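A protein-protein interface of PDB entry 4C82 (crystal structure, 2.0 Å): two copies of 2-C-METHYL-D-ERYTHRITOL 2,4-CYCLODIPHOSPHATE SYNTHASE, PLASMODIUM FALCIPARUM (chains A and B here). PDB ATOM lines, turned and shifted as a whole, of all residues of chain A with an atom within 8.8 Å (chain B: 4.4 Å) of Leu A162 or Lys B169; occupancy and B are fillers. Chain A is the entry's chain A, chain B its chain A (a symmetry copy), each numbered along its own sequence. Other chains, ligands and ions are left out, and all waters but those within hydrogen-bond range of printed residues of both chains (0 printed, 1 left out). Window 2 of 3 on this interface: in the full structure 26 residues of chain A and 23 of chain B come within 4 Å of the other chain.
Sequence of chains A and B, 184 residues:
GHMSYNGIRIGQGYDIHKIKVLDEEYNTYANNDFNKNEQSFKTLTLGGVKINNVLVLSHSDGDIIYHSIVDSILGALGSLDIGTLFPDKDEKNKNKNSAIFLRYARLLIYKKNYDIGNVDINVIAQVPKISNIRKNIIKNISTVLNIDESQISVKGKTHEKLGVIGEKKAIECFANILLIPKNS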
ATOM      1  N   ILE A 124       1.686 -29.052 -10.993  1.00  0.00           N
ATOM      2  CA  ILE A 124       2.456 -27.794 -11.005  1.00  0.00           C
ATOM      3  C   ILE A 124       2.538 -27.421  -9.523  1.00  0.00           C
ATOM      4  O   ILE A 124       1.525 -27.022  -8.863  1.00  0.00           O
ATOM      5  CB  ILE A 124       1.754 -26.698 -11.841  1.00  0.00           C
ATOM      6  CG1 ILE A 124       1.386 -27.289 -13.250  1.00  0.00           C
ATOM      7  CG2 ILE A 124       2.663 -25.435 -11.932  1.00  0.00           C
ATOM      8  CD1 ILE A 124       0.723 -26.313 -14.278  1.00  0.00           C
ATOM      9  N   GLN A 126       5.654 -26.323  -6.483  1.00  0.00           N
ATOM     10  CA  GLN A 126       7.026 -25.974  -6.058  1.00  0.00           C
ATOM     11  C   GLN A 126       7.532 -27.079  -5.140  1.00  0.00           C
ATOM     12  O   GLN A 126       8.659 -27.493  -5.265  1.00  0.00           O
ATOM     13  CB  GLN A 126       7.090 -24.562  -5.365  1.00  0.00           C
ATOM     14  CG  GLN A 126       8.485 -23.935  -5.353  1.00  0.00           C
ATOM     15  CD  GLN A 126       9.077 -23.696  -6.722  1.00  0.00           C
ATOM     16  OE1 GLN A 126       8.395 -23.211  -7.629  1.00  0.00           O
ATOM     17  NE2 GLN A 126      10.375 -23.987  -6.879  1.00  0.00           N
ATOM     18  N   THR A 158       7.978 -27.476 -11.416  1.00  0.00           N
ATOM     19  CA  THR A 158       8.069 -26.326 -10.511  1.00  0.00           C
ATOM     20  C   THR A 158       7.715 -24.990 -11.200  1.00  0.00           C
ATOM     21  O   THR A 158       7.362 -24.939 -12.390  1.00  0.00           O
ATOM     22  CB  THR A 158       9.520 -26.247  -9.942  1.00  0.00           C
ATOM     23  OG1 THR A 158      10.430 -26.314 -11.033  1.00  0.00           O
ATOM     24  CG2 THR A 158       9.799 -27.459  -9.083  1.00  0.00           C
ATOM     25  N   HIS A 159       7.729 -23.887 -10.440  1.00  0.00           N
ATOM     26  CA  HIS A 159       7.080 -22.703 -10.968  1.00  0.00           C
ATOM     27  C   HIS A 159       7.998 -21.557 -10.647  1.00  0.00           C
ATOM     28  O   HIS A 159       7.518 -20.465 -10.270  1.00  0.00           O
ATOM     29  CB  HIS A 159       5.695 -22.509 -10.304  1.00  0.00           C
ATOM     30  CG  HIS A 159       4.777 -21.507 -11.013  1.00  0.00           C
ATOM     31  ND1 HIS A 159       4.693 -20.207 -10.633  1.00  0.00           N
ATOM     32  CD2 HIS A 159       3.837 -21.677 -12.043  1.00  0.00           C
ATOM     33  CE1 HIS A 159       3.825 -19.537 -11.422  1.00  0.00           C
ATOM     34  NE2 HIS A 159       3.286 -20.442 -12.290  1.00  0.00           N
ATOM     35  N   GLU A 160       9.307 -21.825 -10.635  1.00  0.00           N
ATOM     36  CA  GLU A 160      10.311 -20.701 -10.641  1.00  0.00           C
ATOM     37  C   GLU A 160      10.284 -19.846  -9.365  1.00  0.00           C
ATOM     38  O   GLU A 160      10.726 -18.670  -9.364  1.00  0.00           O
ATOM     39  CB  GLU A 160      10.086 -19.838 -11.890  1.00  0.00           C
ATOM     40  CG  GLU A 160      10.220 -20.632 -13.209  1.00  0.00           C
ATOM     41  CD  GLU A 160      11.693 -20.988 -13.478  1.00  0.00           C
ATOM     42  OE1 GLU A 160      12.475 -20.075 -13.736  1.00  0.00           O
ATOM     43  OE2 GLU A 160      12.073 -22.164 -13.404  1.00  0.00           O
ATOM     44  N   LYS A 161       9.688 -20.412  -8.309  1.00  0.00           N
ATOM     45  CA  LYS A 161       9.433 -19.726  -7.057  1.00  0.00           C
ATOM     46  C   LYS A 161       8.720 -18.411  -7.234  1.00  0.00           C
ATOM     47  O   LYS A 161       8.886 -17.501  -6.397  1.00  0.00           O
ATOM     48  CB  LYS A 161      10.763 -19.428  -6.252  1.00  0.00           C
ATOM     49  CG  LYS A 161      11.789 -20.529  -6.305  1.00  0.00           C
ATOM     50  CD  LYS A 161      12.780 -20.448  -5.145  1.00  0.00           C
ATOM     51  CE  LYS A 161      13.385 -21.815  -4.905  1.00  0.00           C
ATOM     52  NZ  LYS A 161      13.886 -21.947  -3.499  1.00  0.00           N
ATOM     53  N   LEU A 162       7.911 -18.288  -8.286  1.00  0.00           N
ATOM     54  CA  LEU A 162       7.102 -17.103  -8.516  1.00  0.00           C
ATOM     55  C   LEU A 162       5.615 -17.419  -8.350  1.00  0.00           C
ATOM     56  O   LEU A 162       5.155 -18.539  -8.664  1.00  0.00           O
ATOM     57  CB  LEU A 162       7.301 -16.619  -9.979  1.00  0.00           C
ATOM     58  CG  LEU A 162       8.722 -16.150 -10.308  1.00  0.00           C
ATOM     59  CD1 LEU A 162       8.767 -15.871 -11.797  1.00  0.00           C
ATOM     60  CD2 LEU A 162       9.129 -14.909  -9.501  1.00  0.00           C
ATOM     61  N   GLY A 163       4.886 -16.422  -7.872  1.00  0.00           N
ATOM     62  CA  GLY A 163       3.446 -16.458  -7.754  1.00  0.00           C
ATOM     63  C   GLY A 163       2.977 -17.361  -6.634  1.00  0.00           C
ATOM     64  O   GLY A 163       3.821 -17.868  -5.867  1.00  0.00           O
ATOM     65  N   VAL A 164       1.657 -17.604  -6.574  1.00  0.00           N
ATOM     66  CA  VAL A 164       1.026 -18.420  -5.490  1.00  0.00           C
ATOM     67  C   VAL A 164       1.651 -19.796  -5.426  1.00  0.00           C
ATOM     68  O   VAL A 164       2.018 -20.247  -4.337  1.00  0.00           O
ATOM     69  CB  VAL A 164      -0.536 -18.561  -5.564  1.00  0.00           C
ATOM     70  CG1 VAL A 164      -1.212 -17.301  -6.025  1.00  0.00           C
ATOM     71  CG2 VAL A 164      -1.004 -19.725  -6.427  1.00  0.00           C
ATOM     72  N   ILE A 165       1.841 -20.429  -6.597  1.00  0.00           N
ATOM     73  CA  ILE A 165       2.431 -21.784  -6.642  1.00  0.00           C
ATOM     74  C   ILE A 165       3.887 -21.749  -6.276  1.00  0.00           C
ATOM     75  O   ILE A 165       4.350 -22.586  -5.512  1.00  0.00           O
ATOM     76  CB  ILE A 165       2.193 -22.536  -7.972  1.00  0.00           C
ATOM     77  CG1 ILE A 165       0.668 -22.864  -8.076  1.00  0.00           C
ATOM     78  CG2 ILE A 165       2.970 -23.863  -8.067  1.00  0.00           C
ATOM     79  CD1 ILE A 165       0.185 -22.586  -9.463  1.00  0.00           C
ATOM     80  N   GLY A 166       4.604 -20.799  -6.839  1.00  0.00           N
ATOM     81  CA  GLY A 166       6.069 -20.819  -6.698  1.00  0.00           C
ATOM     82  C   GLY A 166       6.401 -20.453  -5.240  1.00  0.00           C
ATOM     83  O   GLY A 166       7.424 -20.861  -4.727  1.00  0.00           O
ATOM     84  N   GLU A 167       5.540 -19.686  -4.605  1.00  0.00           N
ATOM     85  CA  GLU A 167       5.702 -19.354  -3.167  1.00  0.00           C
ATOM     86  C   GLU A 167       5.148 -20.425  -2.245  1.00  0.00           C
ATOM     87  O   GLU A 167       5.067 -20.190  -1.056  1.00  0.00           O
ATOM     88  CB  GLU A 167       5.036 -17.999  -2.888  1.00  0.00           C
ATOM     89  CG  GLU A 167       5.845 -16.917  -3.562  1.00  0.00           C
ATOM     90  CD  GLU A 167       5.384 -15.492  -3.263  1.00  0.00           C
ATOM     91  OE1 GLU A 167       4.271 -15.261  -2.729  1.00  0.00           O
ATOM     92  OE2 GLU A 167       6.176 -14.603  -3.613  1.00  0.00           O
ATOM     93  N   LYS A 168       4.756 -21.595  -2.802  1.00  0.00           N
ATOM     94  CA  LYS A 168       4.248 -22.700  -2.007  1.00  0.00           C
ATOM     95  C   LYS A 168       2.986 -22.449  -1.212  1.00  0.00           C
ATOM     96  O   LYS A 168       2.766 -23.115  -0.187  1.00  0.00           O
ATOM     97  CB  LYS A 168       5.327 -23.226  -1.059  1.00  0.00           C
ATOM     98  CG  LYS A 168       6.631 -23.440  -1.748  1.00  0.00           C
ATOM     99  CD  LYS A 168       7.648 -23.940  -0.765  1.00  0.00           C
ATOM    100  CE  LYS A 168       8.977 -23.284  -1.043  1.00  0.00           C
ATOM    101  NZ  LYS A 168      10.074 -24.292  -0.907  1.00  0.00           N
ATOM    102  N   LYS A 169       2.102 -21.606  -1.737  1.00  0.00           N
ATOM    103  CA  LYS A 169       0.842 -21.367  -1.086  1.00  0.00           C
ATOM    104  C   LYS A 169      -0.229 -22.327  -1.605  1.00  0.00           C
ATOM    105  O   LYS A 169      -1.315 -22.383  -1.062  1.00  0.00           O
ATOM    106  CB  LYS A 169       0.373 -19.910  -1.329  1.00  0.00           C
ATOM    107  CG  LYS A 169       1.311 -18.839  -0.747  1.00  0.00           C
ATOM    108  CD  LYS A 169       0.857 -17.420  -1.131  1.00  0.00           C
ATOM    109  CE  LYS A 169       1.758 -16.415  -0.401  1.00  0.00           C
ATOM    110  NZ  LYS A 169       1.185 -15.046  -0.582  1.00  0.00           N
ATOM    111  N   ALA A 170       0.064 -23.016  -2.700  1.00  0.00           N
ATOM    112  CA  ALA A 170      -0.945 -23.829  -3.396  1.00  0.00           C
ATOM    113  C   ALA A 170      -0.218 -24.796  -4.305  1.00  0.00           C
ATOM    114  O   ALA A 170       0.907 -24.540  -4.655  1.00  0.00           O
ATOM    115  CB  ALA A 170      -1.869 -22.931  -4.254  1.00  0.00           C
ATOM    116  N   LYS B  18      11.401 -17.975 -15.963  1.00  0.00           N
ATOM    117  CA  LYS B  18      11.649 -16.559 -15.567  1.00  0.00           C
ATOM    118  C   LYS B  18      12.324 -15.733 -16.659  1.00  0.00           C
ATOM    119  O   LYS B  18      13.287 -16.202 -17.296  1.00  0.00           O
ATOM    120  CB  LYS B  18      12.577 -16.531 -14.332  1.00  0.00           C
ATOM    121  CG  LYS B  18      11.932 -17.100 -13.101  1.00  0.00           C
ATOM    122  CD  LYS B  18      12.877 -17.220 -11.887  1.00  0.00           C
ATOM    123  CE  LYS B  18      13.762 -16.002 -11.737  1.00  0.00           C
ATOM    124  NZ  LYS B  18      12.993 -14.731 -11.643  1.00  0.00           N
ATOM    125  N   ILE B  19      11.860 -14.495 -16.848  1.00  0.00           N
ATOM    126  CA  ILE B  19      12.405 -13.642 -17.872  1.00  0.00           C
ATOM    127  C   ILE B  19      12.688 -12.246 -17.289  1.00  0.00           C
ATOM    128  O   ILE B  19      12.212 -11.904 -16.210  1.00  0.00           O
ATOM    129  CB  ILE B  19      11.467 -13.476 -19.067  1.00  0.00           C
ATOM    130  CG1 ILE B  19      10.082 -13.004 -18.604  1.00  0.00           C
ATOM    131  CG2 ILE B  19      11.383 -14.784 -19.871  1.00  0.00           C
ATOM    132  CD1 ILE B  19       9.369 -12.277 -19.750  1.00  0.00           C
ATOM    133  N   VAL B 164       2.187 -12.832 -12.162  1.00  0.00           N
ATOM    134  CA  VAL B 164       3.620 -13.058 -12.528  1.00  0.00           C
ATOM    135  C   VAL B 164       3.819 -12.912 -14.020  1.00  0.00           C
ATOM    136  O   VAL B 164       4.741 -12.208 -14.444  1.00  0.00           O
ATOM    137  CB  VAL B 164       4.239 -14.420 -12.051  1.00  0.00           C
ATOM    138  CG1 VAL B 164       3.751 -14.835 -10.691  1.00  0.00           C
ATOM    139  CG2 VAL B 164       4.024 -15.565 -13.032  1.00  0.00           C
ATOM    140  N   GLU B 167       2.901  -9.280 -15.351  1.00  0.00           N
ATOM    141  CA  GLU B 167       3.979  -8.347 -14.939  1.00  0.00           C
ATOM    142  C   GLU B 167       5.315  -8.663 -15.586  1.00  0.00           C
ATOM    143  O   GLU B 167       6.307  -8.080 -15.197  1.00  0.00           O
ATOM    144  CB  GLU B 167       4.099  -8.365 -13.408  1.00  0.00           C
ATOM    145  CG  GLU B 167       2.869  -7.715 -12.821  1.00  0.00           C
ATOM    146  CD  GLU B 167       2.902  -7.534 -11.305  1.00  0.00           C
ATOM    147  OE1 GLU B 167       3.753  -8.121 -10.592  1.00  0.00           O
ATOM    148  OE2 GLU B 167       2.016  -6.795 -10.848  1.00  0.00           O
ATOM    149  N   LYS B 168       5.336  -9.598 -16.566  1.00  0.00           N
ATOM    150  CA  LYS B 168       6.553  -9.948 -17.277  1.00  0.00           C
ATOM    151  C   LYS B 168       7.684 -10.524 -16.457  1.00  0.00           C
ATOM    152  O   LYS B 168       8.854 -10.397 -16.854  1.00  0.00           O
ATOM    153  CB  LYS B 168       7.081  -8.749 -18.068  1.00  0.00           C
ATOM    154  CG  LYS B 168       6.014  -8.076 -18.858  1.00  0.00           C
ATOM    155  CD  LYS B 168       6.591  -6.904 -19.596  1.00  0.00           C
ATOM    156  CE  LYS B 168       5.613  -5.756 -19.554  1.00  0.00           C
ATOM    157  NZ  LYS B 168       5.574  -5.081 -20.888  1.00  0.00           N
ATOM    158  N   LYS B 169       7.349 -11.263 -15.404  1.00  0.00           N
ATOM    159  CA  LYS B 169       8.360 -11.912 -14.612  1.00  0.00           C
ATOM    160  C   LYS B 169       8.631 -13.326 -15.128  1.00  0.00           C
ATOM    161  O   LYS B 169       9.562 -13.969 -14.687  1.00  0.00           O
ATOM    162  CB  LYS B 169       7.917 -11.993 -13.128  1.00  0.00           C
ATOM    163  CG  LYS B 169       7.724 -10.626 -12.451  1.00  0.00           C
ATOM    164  CD  LYS B 169       7.164 -10.775 -11.025  1.00  0.00           C
ATOM    165  CE  LYS B 169       7.133  -9.385 -10.376  1.00  0.00           C
ATOM    166  NZ  LYS B 169       6.813  -9.546  -8.925  1.00  0.00           N
ATOM    167  N   ALA B 170       7.764 -13.821 -16.003  1.00  0.00           N
ATOM    168  CA  ALA B 170       7.815 -15.225 -16.431  1.00  0.00           C
ATOM    169  C   ALA B 170       7.012 -15.354 -17.708  1.00  0.00           C
ATOM    170  O   ALA B 170       6.173 -14.524 -17.959  1.00  0.00           O
ATOM    171  CB  ALA B 170       7.191 -16.145 -15.352  1.00  0.00           C
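5 positions are printed for both chains.
Of the 6 pairs that touch across the chains among the printed residues, none has its exchanged pair printed and touching as well.
The side-chain carboxylate (OE1) of Glu A160 lies close to the backbone NH (N) of Lys B18 (3.2 Å).
Ile A124 touches none of the printed residues of chain B.
Of the printed residues of chain B, Glu A160 touches Lys B18.
Of chain B, only Lys B18 (3.6 Å), Val B164 (3.95 Å), Lys B169 (3.5 Å) and Ala B170 (3.9 Å) come within 4 Å of Leu A162.
Of the printed residues of chain A, Lys B18 touches Glu A160 (3.1 Å) and Leu A162 (3.6 Å).
Of the printed residues of chain A, Val B164 touches Leu A162 and Gly A163.
Ala B170 touches just one residue of chain A: Leu A162 (3.9 Å).
The nearest residue of chain A that does not touch Lys B169 is Glu A160 (6.5 Å).
The backbone carbonyl oxygen (O) of Lys B169 sits at hydrogen-bond distance from the backbone NH (N) of Ile B19.
The backbone carbonyl oxygen (O) of Val B164 lies within hydrogen-bond range of the backbone NH (N) of Lys B169 (2.9 Å).
A ring nitrogen (ND1) of His A159 sits at hydrogen-bond distance from the backbone carbonyl oxygen of Leu A162 (2.6 Å).
The side-chain amino group (NZ) of Lys B169 lies within salt-bridge range of the side-chain carboxylate (OE1) of Glu B167 (3.8 Å).
OE1 of Gln A126 sits at hydrogen-bond distance from N of Glu A160, at 3.4 Å.
Among the printed residues, merely in contact across the chains: Leu A162 with Lys B18 (3.6 Å), Leu A162 with Val B164 (3.95 Å), Leu A162 with Lys B169 (3.5 Å), Leu A162 with Ala B170 (3.9 Å) and Gly A163 with Val B164 (3.4 Å).
Hydrophobic or aromatic side chains of chain B that line the printed part of chain A: Val B164 and Ala B170.
Of the 15 printed residues of chain A, 3 touch a printed residue of chain B.
Printed residues of chain A that touch a printed residue of chain B: Glu A160, Leu A162 and Gly A163.
Hydrophobic or aromatic side chains of chain A that line the printed part of chain B: Leu A162.
Among the printed residues, 6 pairs touch across the chains.
Among the printed residues, no Asp or Glu carboxylate lies within 4 Å of a Lys or Arg side-chain nitrogen of the other chain.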
